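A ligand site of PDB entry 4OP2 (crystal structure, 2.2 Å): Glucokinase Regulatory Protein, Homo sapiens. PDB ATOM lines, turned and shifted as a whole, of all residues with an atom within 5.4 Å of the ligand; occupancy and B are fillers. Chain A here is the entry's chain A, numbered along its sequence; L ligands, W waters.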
ATOM      1  N   HIS A  21       3.727   9.136  17.988  1.00  0.00           N
ATOM      2  CA  HIS A  21       3.947  10.504  18.394  1.00  0.00           C
ATOM      3  C   HIS A  21       4.555  10.635  19.840  1.00  0.00           C
ATOM      4  O   HIS A  21       4.947  11.702  20.269  1.00  0.00           O
ATOM      5  CB  HIS A  21       2.632  11.236  18.326  1.00  0.00           C
ATOM      6  CG  HIS A  21       1.668  10.753  19.358  1.00  0.00           C
ATOM      7  ND1 HIS A  21       0.886   9.633  19.178  1.00  0.00           N
ATOM      8  CD2 HIS A  21       1.450  11.167  20.635  1.00  0.00           C
ATOM      9  CE1 HIS A  21       0.171   9.420  20.261  1.00  0.00           C
ATOM     10  NE2 HIS A  21       0.484  10.344  21.156  1.00  0.00           N
ATOM     11  N   TRP A  31      16.476  14.912  31.174  1.00  0.00           N
ATOM     12  CA  TRP A  31      15.102  15.351  30.875  1.00  0.00           C
ATOM     13  C   TRP A  31      15.059  16.711  30.148  1.00  0.00           C
ATOM     14  O   TRP A  31      14.298  16.900  29.198  1.00  0.00           O
ATOM     15  CB  TRP A  31      14.296  15.366  32.160  1.00  0.00           C
ATOM     16  CG  TRP A  31      13.811  14.010  32.540  1.00  0.00           C
ATOM     17  CD1 TRP A  31      14.461  13.080  33.314  1.00  0.00           C
ATOM     18  CD2 TRP A  31      12.569  13.402  32.146  1.00  0.00           C
ATOM     19  NE1 TRP A  31      13.690  11.921  33.421  1.00  0.00           N
ATOM     20  CE2 TRP A  31      12.532  12.099  32.710  1.00  0.00           C
ATOM     21  CE3 TRP A  31      11.479  13.826  31.355  1.00  0.00           C
ATOM     22  CZ2 TRP A  31      11.451  11.253  32.532  1.00  0.00           C
ATOM     23  CZ3 TRP A  31      10.413  12.950  31.160  1.00  0.00           C
ATOM     24  CH2 TRP A  31      10.399  11.694  31.762  1.00  0.00           C
ATOM     25  N   TYR A  36      12.731  16.154  25.213  1.00  0.00           N
ATOM     26  CA  TYR A  36      11.428  15.637  25.558  1.00  0.00           C
ATOM     27  C   TYR A  36      10.663  16.861  26.089  1.00  0.00           C
ATOM     28  O   TYR A  36       9.624  17.238  25.541  1.00  0.00           O
ATOM     29  CB  TYR A  36      11.552  14.567  26.632  1.00  0.00           C
ATOM     30  CG  TYR A  36      10.237  14.006  27.085  1.00  0.00           C
ATOM     31  CD1 TYR A  36       9.485  14.670  28.046  1.00  0.00           C
ATOM     32  CD2 TYR A  36       9.735  12.841  26.549  1.00  0.00           C
ATOM     33  CE1 TYR A  36       8.259  14.175  28.471  1.00  0.00           C
ATOM     34  CE2 TYR A  36       8.510  12.342  26.966  1.00  0.00           C
ATOM     35  CZ  TYR A  36       7.783  13.028  27.931  1.00  0.00           C
ATOM     36  OH  TYR A  36       6.578  12.593  28.388  1.00  0.00           O
ATOM     37  N   GLU A  37      11.243  17.521  27.096  1.00  0.00           N
ATOM     38  CA  GLU A  37      10.673  18.722  27.715  1.00  0.00           C
ATOM     39  C   GLU A  37      10.229  19.808  26.714  1.00  0.00           C
ATOM     40  O   GLU A  37       9.179  20.419  26.869  1.00  0.00           O
ATOM     41  CB  GLU A  37      11.682  19.327  28.662  1.00  0.00           C
ATOM     42  CG  GLU A  37      11.155  19.668  30.032  1.00  0.00           C
ATOM     43  CD  GLU A  37      11.044  18.467  30.927  1.00  0.00           C
ATOM     44  OE1 GLU A  37      11.818  18.341  31.906  1.00  0.00           O
ATOM     45  OE2 GLU A  37      10.149  17.631  30.652  1.00  0.00           O
ATOM     46  N   VAL A  40       6.873  19.126  25.321  1.00  0.00           N
ATOM     47  CA  VAL A  40       5.646  18.976  26.156  1.00  0.00           C
ATOM     48  C   VAL A  40       4.876  20.251  25.949  1.00  0.00           C
ATOM     49  O   VAL A  40       5.398  21.343  26.199  1.00  0.00           O
ATOM     50  CB  VAL A  40       5.906  18.782  27.671  1.00  0.00           C
ATOM     51  CG1 VAL A  40       4.588  18.833  28.475  1.00  0.00           C
ATOM     52  CG2 VAL A  40       6.612  17.479  27.958  1.00  0.00           C
ATOM     53  N   PRO A  41       3.631  20.149  25.477  1.00  0.00           N
ATOM     54  CA  PRO A  41       2.895  21.400  25.275  1.00  0.00           C
ATOM     55  C   PRO A  41       2.826  22.266  26.535  1.00  0.00           C
ATOM     56  O   PRO A  41       2.766  21.764  27.660  1.00  0.00           O
ATOM     57  CB  PRO A  41       1.517  20.931  24.839  1.00  0.00           C
ATOM     58  CG  PRO A  41       1.693  19.532  24.368  1.00  0.00           C
ATOM     59  CD  PRO A  41       2.809  18.959  25.155  1.00  0.00           C
ATOM     60  N   THR A  43       0.564  23.608  27.943  1.00  0.00           N
ATOM     61  CA  THR A  43      -0.617  23.382  28.765  1.00  0.00           C
ATOM     62  C   THR A  43      -0.485  22.149  29.603  1.00  0.00           C
ATOM     63  O   THR A  43      -1.137  22.043  30.602  1.00  0.00           O
ATOM     64  CB  THR A  43      -1.909  23.281  27.927  1.00  0.00           C
ATOM     65  OG1 THR A  43      -1.762  22.318  26.893  1.00  0.00           O
ATOM     66  CG2 THR A  43      -2.221  24.653  27.261  1.00  0.00           C
ATOM     67  N   GLU A  44       0.357  21.209  29.165  1.00  0.00           N
ATOM     68  CA  GLU A  44       0.630  19.999  29.883  1.00  0.00           C
ATOM     69  C   GLU A  44       1.829  20.078  30.793  1.00  0.00           C
ATOM     70  O   GLU A  44       2.050  19.138  31.511  1.00  0.00           O
ATOM     71  CB  GLU A  44       0.810  18.799  28.908  1.00  0.00           C
ATOM     72  CG  GLU A  44      -0.466  18.574  28.119  1.00  0.00           C
ATOM     73  CD  GLU A  44      -1.637  18.039  28.930  1.00  0.00           C
ATOM     74  OE1 GLU A  44      -1.408  17.376  29.944  1.00  0.00           O
ATOM     75  OE2 GLU A  44      -2.794  18.306  28.557  1.00  0.00           O
ATOM     76  N   LYS A  45       2.564  21.170  30.789  1.00  0.00           N
ATOM     77  CA  LYS A  45       3.835  21.195  31.547  1.00  0.00           C
ATOM     78  C   LYS A  45       3.574  21.230  33.059  1.00  0.00           C
ATOM     79  O   LYS A  45       2.496  21.645  33.523  1.00  0.00           O
ATOM     80  CB  LYS A  45       4.694  22.407  31.140  1.00  0.00           C
ATOM     81  CG  LYS A  45       5.511  22.285  29.828  1.00  0.00           C
ATOM     82  CD  LYS A  45       6.357  23.562  29.623  1.00  0.00           C
ATOM     83  CE  LYS A  45       6.848  23.839  28.205  1.00  0.00           C
ATOM     84  NZ  LYS A  45       7.506  22.665  27.588  1.00  0.00           N
ATOM     85  N   SER A  46       4.602  20.812  33.803  1.00  0.00           N
ATOM     86  CA  SER A  46       4.710  21.011  35.234  1.00  0.00           C
ATOM     87  C   SER A  46       5.067  22.484  35.525  1.00  0.00           C
ATOM     88  O   SER A  46       6.083  22.955  35.064  1.00  0.00           O
ATOM     89  CB  SER A  46       5.830  20.112  35.826  1.00  0.00           C
ATOM     90  OG  SER A  46       6.086  20.414  37.201  1.00  0.00           O
ATOM     91  N   GLY A 193      -5.853  23.457  25.158  1.00  0.00           N
ATOM     92  CA  GLY A 193      -4.721  22.723  24.706  1.00  0.00           C
ATOM     93  C   GLY A 193      -4.511  22.716  23.206  1.00  0.00           C
ATOM     94  O   GLY A 193      -3.516  22.111  22.760  1.00  0.00           O
ATOM     95  N   LEU A 194      -5.354  23.398  22.426  1.00  0.00           N
ATOM     96  CA  LEU A 194      -5.415  23.191  20.962  1.00  0.00           C
ATOM     97  C   LEU A 194      -5.447  21.652  20.689  1.00  0.00           C
ATOM     98  O   LEU A 194      -4.589  21.051  19.996  1.00  0.00           O
ATOM     99  CB  LEU A 194      -4.229  23.842  20.301  1.00  0.00           C
ATOM    100  CG  LEU A 194      -4.050  25.384  20.330  1.00  0.00           C
ATOM    101  CD1 LEU A 194      -2.977  25.830  19.310  1.00  0.00           C
ATOM    102  CD2 LEU A 194      -5.339  26.059  19.958  1.00  0.00           C
ATOM    103  N   SER A 195      -6.411  21.020  21.322  1.00  0.00           N
ATOM    104  CA  SER A 195      -6.411  19.589  21.517  1.00  0.00           C
ATOM    105  C   SER A 195      -7.731  18.911  21.121  1.00  0.00           C
ATOM    106  O   SER A 195      -7.705  17.814  20.607  1.00  0.00           O
ATOM    107  CB  SER A 195      -6.173  19.274  23.007  1.00  0.00           C
ATOM    108  OG  SER A 195      -6.812  18.041  23.338  1.00  0.00           O
ATOM    109  N   ASN A 221      -1.522  27.309  23.461  1.00  0.00           N
ATOM    110  CA  ASN A 221      -0.240  26.767  23.067  1.00  0.00           C
ATOM    111  C   ASN A 221       0.121  27.410  21.760  1.00  0.00           C
ATOM    112  O   ASN A 221      -0.746  27.734  20.974  1.00  0.00           O
ATOM    113  CB  ASN A 221      -0.337  25.286  22.824  1.00  0.00           C
ATOM    114  CG  ASN A 221      -0.318  24.482  24.069  1.00  0.00           C
ATOM    115  OD1 ASN A 221       0.509  24.680  24.940  1.00  0.00           O
ATOM    116  ND2 ASN A 221      -1.253  23.544  24.169  1.00  0.00           N
ATOM    117  N   MET A 225       2.909  23.455  18.897  1.00  0.00           N
ATOM    118  CA  MET A 225       2.702  22.506  19.982  1.00  0.00           C
ATOM    119  C   MET A 225       1.292  21.959  19.966  1.00  0.00           C
ATOM    120  O   MET A 225       0.877  21.274  20.917  1.00  0.00           O
ATOM    121  CB  MET A 225       2.931  23.167  21.363  1.00  0.00           C
ATOM    122  CG  MET A 225       4.342  23.130  21.862  1.00  0.00           C
ATOM    123  SD  MET A 225       4.589  24.326  23.188  1.00  0.00           S
ATOM    124  CE  MET A 225       6.214  23.784  23.733  1.00  0.00           C
ATOM    125  N   ALA A 226       0.530  22.277  18.934  1.00  0.00           N
ATOM    126  CA  ALA A 226      -0.849  21.805  18.866  1.00  0.00           C
ATOM    127  C   ALA A 226      -0.886  20.327  18.687  1.00  0.00           C
ATOM    128  O   ALA A 226      -0.020  19.762  18.079  1.00  0.00           O
ATOM    129  CB  ALA A 226      -1.598  22.429  17.739  1.00  0.00           C
ATOM    130  N   ARG A 227      -1.956  19.725  19.177  1.00  0.00           N
ATOM    131  CA  ARG A 227      -2.087  18.289  19.185  1.00  0.00           C
ATOM    132  C   ARG A 227      -1.974  17.724  17.805  1.00  0.00           C
ATOM    133  O   ARG A 227      -2.591  18.218  16.849  1.00  0.00           O
ATOM    134  CB  ARG A 227      -3.408  17.916  19.762  1.00  0.00           C
ATOM    135  CG  ARG A 227      -3.349  16.593  20.363  1.00  0.00           C
ATOM    136  CD  ARG A 227      -4.528  16.361  21.288  1.00  0.00           C
ATOM    137  NE  ARG A 227      -4.777  14.935  21.294  1.00  0.00           N
ATOM    138  CZ  ARG A 227      -5.777  14.335  21.940  1.00  0.00           C
ATOM    139  NH1 ARG A 227      -6.616  15.064  22.677  1.00  0.00           N
ATOM    140  NH2 ARG A 227      -5.924  13.004  21.841  1.00  0.00           N
ATOM    141  N   ASN A 228      -1.186  16.650  17.732  1.00  0.00           N
ATOM    142  CA  ASN A 228      -0.861  16.014  16.453  1.00  0.00           C
ATOM    143  C   ASN A 228      -1.025  14.492  16.362  1.00  0.00           C
ATOM    144  O   ASN A 228      -0.613  13.925  15.401  1.00  0.00           O
ATOM    145  CB  ASN A 228       0.567  16.461  15.984  1.00  0.00           C
ATOM    146  CG  ASN A 228       0.784  16.248  14.502  1.00  0.00           C
ATOM    147  OD1 ASN A 228      -0.008  16.685  13.643  1.00  0.00           O
ATOM    148  ND2 ASN A 228       1.832  15.528  14.175  1.00  0.00           N
ATOM    149  N   ASP A 229      -1.665  13.837  17.328  1.00  0.00           N
ATOM    150  CA  ASP A 229      -2.009  12.415  17.216  1.00  0.00           C
ATOM    151  C   ASP A 229      -3.316  12.258  16.447  1.00  0.00           C
ATOM    152  O   ASP A 229      -4.145  13.171  16.453  1.00  0.00           O
ATOM    153  CB  ASP A 229      -2.057  11.709  18.605  1.00  0.00           C
ATOM    154  CG  ASP A 229      -3.009  12.381  19.607  1.00  0.00           C
ATOM    155  OD1 ASP A 229      -2.834  13.585  19.925  1.00  0.00           O
ATOM    156  OD2 ASP A 229      -3.907  11.707  20.148  1.00  0.00           O
ATOM    157  N   SER A 267      -0.858  20.542  37.085  1.00  0.00           N
ATOM    158  CA  SER A 267      -0.487  20.181  35.732  1.00  0.00           C
ATOM    159  C   SER A 267      -1.647  19.701  34.902  1.00  0.00           C
ATOM    160  O   SER A 267      -2.330  18.758  35.269  1.00  0.00           O
ATOM    161  CB  SER A 267       0.630  19.138  35.744  1.00  0.00           C
ATOM    162  OG  SER A 267       1.668  19.471  36.710  1.00  0.00           O
ATOM    163  N   HIS A 516       0.946  16.967  40.147  1.00  0.00           N
ATOM    164  CA  HIS A 516       0.263  16.089  39.224  1.00  0.00           C
ATOM    165  C   HIS A 516      -0.880  15.352  39.954  1.00  0.00           C
ATOM    166  O   HIS A 516      -0.770  15.008  41.158  1.00  0.00           O
ATOM    167  CB  HIS A 516       1.260  15.071  38.670  1.00  0.00           C
ATOM    168  CG  HIS A 516       2.433  15.699  37.950  1.00  0.00           C
ATOM    169  ND1 HIS A 516       2.295  16.426  36.788  1.00  0.00           N
ATOM    170  CD2 HIS A 516       3.766  15.686  38.235  1.00  0.00           C
ATOM    171  CE1 HIS A 516       3.484  16.822  36.368  1.00  0.00           C
ATOM    172  NE2 HIS A 516       4.394  16.404  37.238  1.00  0.00           N
ATOM    173  N   SER A 525      -9.075  10.485  25.213  1.00  0.00           N
ATOM    174  CA  SER A 525      -7.768  10.171  24.674  1.00  0.00           C
ATOM    175  C   SER A 525      -6.654  11.066  25.292  1.00  0.00           C
ATOM    176  O   SER A 525      -5.561  10.608  25.609  1.00  0.00           O
ATOM    177  CB  SER A 525      -7.810  10.295  23.160  1.00  0.00           C
ATOM    178  OG  SER A 525      -8.179  11.630  22.714  1.00  0.00           O
ATOM    179  N   LYS A 526      -6.946  12.353  25.483  1.00  0.00           N
ATOM    180  CA  LYS A 526      -5.986  13.243  26.134  1.00  0.00           C
ATOM    181  C   LYS A 526      -5.576  12.772  27.502  1.00  0.00           C
ATOM    182  O   LYS A 526      -4.387  12.798  27.856  1.00  0.00           O
ATOM    183  CB  LYS A 526      -6.555  14.672  26.213  1.00  0.00           C
ATOM    184  CG  LYS A 526      -5.716  15.632  27.034  1.00  0.00           C
ATOM    185  CD  LYS A 526      -6.219  17.086  26.912  1.00  0.00           C
ATOM    186  CE  LYS A 526      -7.509  17.319  27.670  1.00  0.00           C
ATOM    187  NZ  LYS A 526      -8.050  18.565  27.158  1.00  0.00           N
ATOM    188  N   TRP A 529      -3.196  10.021  27.179  1.00  0.00           N
ATOM    189  CA  TRP A 529      -1.790  10.463  26.952  1.00  0.00           C
ATOM    190  C   TRP A 529      -1.219  11.032  28.166  1.00  0.00           C
ATOM    191  O   TRP A 529      -0.044  10.818  28.428  1.00  0.00           O
ATOM    192  CB  TRP A 529      -1.646  11.434  25.757  1.00  0.00           C
ATOM    193  CG  TRP A 529      -2.172  10.820  24.549  1.00  0.00           C
ATOM    194  CD1 TRP A 529      -3.228  11.228  23.827  1.00  0.00           C
ATOM    195  CD2 TRP A 529      -1.730   9.597  23.964  1.00  0.00           C
ATOM    196  NE1 TRP A 529      -3.460  10.340  22.796  1.00  0.00           N
ATOM    197  CE2 TRP A 529      -2.531   9.348  22.853  1.00  0.00           C
ATOM    198  CE3 TRP A 529      -0.674   8.725  24.232  1.00  0.00           C
ATOM    199  CZ2 TRP A 529      -2.344   8.250  22.000  1.00  0.00           C
ATOM    200  CZ3 TRP A 529      -0.477   7.584  23.355  1.00  0.00           C
ATOM    201  CH2 TRP A 529      -1.332   7.369  22.298  1.00  0.00           C
ATOM    202  N   ARG A 530      -2.039  11.764  28.950  1.00  0.00           N
ATOM    203  CA  ARG A 530      -1.532  12.313  30.229  1.00  0.00           C
ATOM    204  C   ARG A 530      -1.084  11.199  31.155  1.00  0.00           C
ATOM    205  O   ARG A 530      -0.069  11.318  31.860  1.00  0.00           O
ATOM    206  CB  ARG A 530      -2.547  13.201  30.930  1.00  0.00           C
ATOM    207  CG  ARG A 530      -1.943  13.964  32.104  1.00  0.00           C
ATOM    208  CD  ARG A 530      -2.858  15.049  32.619  1.00  0.00           C
ATOM    209  NE  ARG A 530      -3.234  15.979  31.535  1.00  0.00           N
ATOM    210  CZ  ARG A 530      -4.448  16.543  31.383  1.00  0.00           C
ATOM    211  NH1 ARG A 530      -5.384  16.281  32.251  1.00  0.00           N
ATOM    212  NH2 ARG A 530      -4.738  17.355  30.367  1.00  0.00           N
ATOM    213  N   ALA A 533       2.331   9.666  29.838  1.00  0.00           N
ATOM    214  CA  ALA A 533       3.292  10.692  30.247  1.00  0.00           C
ATOM    215  C   ALA A 533       3.660  10.637  31.761  1.00  0.00           C
ATOM    216  O   ALA A 533       4.854  10.691  32.170  1.00  0.00           O
ATOM    217  CB  ALA A 533       2.748  12.040  29.878  1.00  0.00           C
ATOM    218  N   MET A 534       2.648  10.528  32.613  1.00  0.00           N
ATOM    219  CA  MET A 534       2.902  10.527  34.038  1.00  0.00           C
ATOM    220  C   MET A 534       3.624   9.242  34.453  1.00  0.00           C
ATOM    221  O   MET A 534       4.520   9.272  35.280  1.00  0.00           O
ATOM    222  CB  MET A 534       1.620  10.718  34.805  1.00  0.00           C
ATOM    223  CG  MET A 534       1.214  12.171  34.856  1.00  0.00           C
ATOM    224  SD  MET A 534      -0.177  12.394  35.970  1.00  0.00           S
ATOM    225  CE  MET A 534      -1.391  11.427  35.145  1.00  0.00           C
ATOM    226  N   ARG A 537       7.317   9.782  33.538  1.00  0.00           N
ATOM    227  CA  ARG A 537       7.971  10.735  34.431  1.00  0.00           C
ATOM    228  C   ARG A 537       8.235  10.132  35.814  1.00  0.00           C
ATOM    229  O   ARG A 537       9.294  10.302  36.346  1.00  0.00           O
ATOM    230  CB  ARG A 537       7.144  12.029  34.574  1.00  0.00           C
ATOM    231  CG  ARG A 537       7.688  13.048  35.609  1.00  0.00           C
ATOM    232  CD  ARG A 537       8.895  13.872  35.161  1.00  0.00           C
ATOM    233  NE  ARG A 537       8.529  14.793  34.071  1.00  0.00           N
ATOM    234  CZ  ARG A 537       9.349  15.649  33.444  1.00  0.00           C
ATOM    235  NH1 ARG A 537      10.616  15.742  33.824  1.00  0.00           N
ATOM    236  NH2 ARG A 537       8.892  16.425  32.450  1.00  0.00           N
HETATM  237  C1  LIG L   1      -2.448  17.417  24.300  1.00  0.00           C
HETATM  238  C2  LIG L   1      -2.427  18.712  23.904  1.00  0.00           C
HETATM  239  C3  LIG L   1      -1.478  19.077  22.946  1.00  0.00           C
HETATM  240  N1  LIG L   1      -1.496  20.318  22.536  1.00  0.00           N
HETATM  241  N2  LIG L   1      -0.623  18.164  22.431  1.00  0.00           N
HETATM  242  C4  LIG L   1      -0.650  16.898  22.823  1.00  0.00           C
HETATM  243  C5  LIG L   1      -1.579  16.491  23.737  1.00  0.00           C
HETATM  244  S1  LIG L   1      -1.600  14.883  24.390  1.00  0.00           S
HETATM  245  O1  LIG L   1      -3.001  14.587  24.828  1.00  0.00           O
HETATM  246  O2  LIG L   1      -1.023  13.988  23.430  1.00  0.00           O
HETATM  247  C6  LIG L   1      -0.609  14.980  25.737  1.00  0.00           C
HETATM  248  C7  LIG L   1       0.747  15.246  25.528  1.00  0.00           C
HETATM  249  C8  LIG L   1       1.617  15.346  26.619  1.00  0.00           C
HETATM  250  C9  LIG L   1      -1.097  14.806  27.006  1.00  0.00           C
HETATM  251  C10 LIG L   1      -0.228  14.943  28.092  1.00  0.00           C
HETATM  252  C11 LIG L   1       1.149  15.203  27.911  1.00  0.00           C
HETATM  253  C12 LIG L   1       2.030  15.314  29.021  1.00  0.00           C
HETATM  254  C13 LIG L   1       3.413  15.377  28.844  1.00  0.00           C
HETATM  255  C14 LIG L   1       4.289  15.448  29.938  1.00  0.00           C
HETATM  256  C15 LIG L   1       1.555  15.392  30.343  1.00  0.00           C
HETATM  257  C16 LIG L   1       2.430  15.504  31.441  1.00  0.00           C
HETATM  258  C17 LIG L   1       3.801  15.527  31.236  1.00  0.00           C
HETATM  259  C18 LIG L   1       4.776  15.655  32.409  1.00  0.00           C
HETATM  260  C19 LIG L   1       4.506  14.711  33.560  1.00  0.00           C
HETATM  261  F1  LIG L   1       3.381  15.034  34.147  1.00  0.00           F
HETATM  262  F2  LIG L   1       4.472  13.463  33.118  1.00  0.00           F
HETATM  263  F3  LIG L   1       5.516  14.871  34.413  1.00  0.00           F
HETATM  264  C20 LIG L   1       4.781  17.114  32.916  1.00  0.00           C
HETATM  265  O3  LIG L   1       6.036  15.181  32.015  1.00  0.00           O
HETATM  266  O   HOH W   1       1.728  17.990  21.009  1.00  0.00           O
HETATM  267  O   HOH W   2      -3.384  20.280  26.852  1.00  0.00           O
HETATM  268  O   HOH W   3       6.423  12.605  31.010  1.00  0.00           O
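NH2 of Arg 537 sits at hydrogen-bond distance from O3 of the ligand. The backbone carbonyl oxygen (O) of Met 225 sits at hydrogen-bond distance from a nitrogen (N1) of the ligand, at 3.0 Å. A nitrogen (N1) of the ligand lies within hydrogen-bond range of the backbone carbonyl oxygen (O) of Gly 193 (2.7 Å).
The backbone NH of Arg 227 sits close to a nitrogen (N1) of the ligand (3.4 Å). ND1 of His 516 lies close to F1 of the ligand (3.2 Å). The backbone carbonyl oxygen (O) of Ala 533 lies close to a fluorine (F2) of the ligand (3.0 Å). The backbone NH (N) of Met 534 sits close to a fluorine (F2) of the ligand, 3.5 Å away. Tyr 36 touches the ligand. Val 40 touches the ligand (CG2 to C14, 3.7 Å). CG of Pro 41 touches N2 of the ligand, at 3.3 Å. Glu 44 touches the ligand (OE1 to C10, 3.3 Å). Ser 46 touches the ligand (N to C20, 3.8 Å). Ser 195 touches the ligand. Asn 221 touches the ligand (ND2 to N1, 3.6 Å). Ala 226 touches the ligand. Asp 229 touches the ligand. Lys 526 touches the ligand. Trp 529 touches the ligand. CA of Arg 530 touches C10 of the ligand, 3.6 Å away. Hydrophobic or aromatic side chains that line the ligand: Val 40, Pro 41, His 516, Trp 529, Ala 533 and Met 534. Within 4 Å of the ligand: Tyr 36, Val 40, Pro 41, Glu 44, Ser 46, Gly 193, Ser 195, Asn 221, Met 225, Ala 226, Arg 227, Asp 229, His 516, Lys 526, Trp 529, Arg 530, Ala 533, Met 534 and Arg 537.
O of Val 40 lies within hydrogen-bond range of NZ of Lys 45. OG of Ser 195 is in hydrogen-bond range of NH1 of Arg 227 (3.1 Å). The side-chain hydroxyl (OG1) of Thr 43 lies within hydrogen-bond range of the side-chain amide nitrogen (ND2) of Asn 221, 3.0 Å away. The guanidinium group (NE) of Arg 227 is in salt-bridge range of the side-chain carboxylate (OD1) of Asp 229, 2.7 Å away. The guanidinium group of Arg 530 lies within salt-bridge range of the side-chain carboxylate of Glu 44. N of Arg 227 sits at hydrogen-bond distance from O of Leu 194, 3.1 Å away. NH2 of Arg 537 is in salt-bridge range of OE2 of Glu 37 (2.5 Å). The side-chain hydroxyl (OG) of Ser 267 is in hydrogen-bond range of a ring nitrogen (ND1) of His 516 (3.1 Å).
Water W1 bridges a nitrogen (N2) of the ligand and the backbone carbonyl oxygen (O) of Met 225. Water W3 lies within hydrogen-bond range of OH of Tyr 36 (2.6 Å), O of Ala 533 (2.7 Å) and O3 of the ligand (2.8 Å). Water W2 lies within hydrogen-bond range of OG1 of Thr 43 and OE2 of Glu 44.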
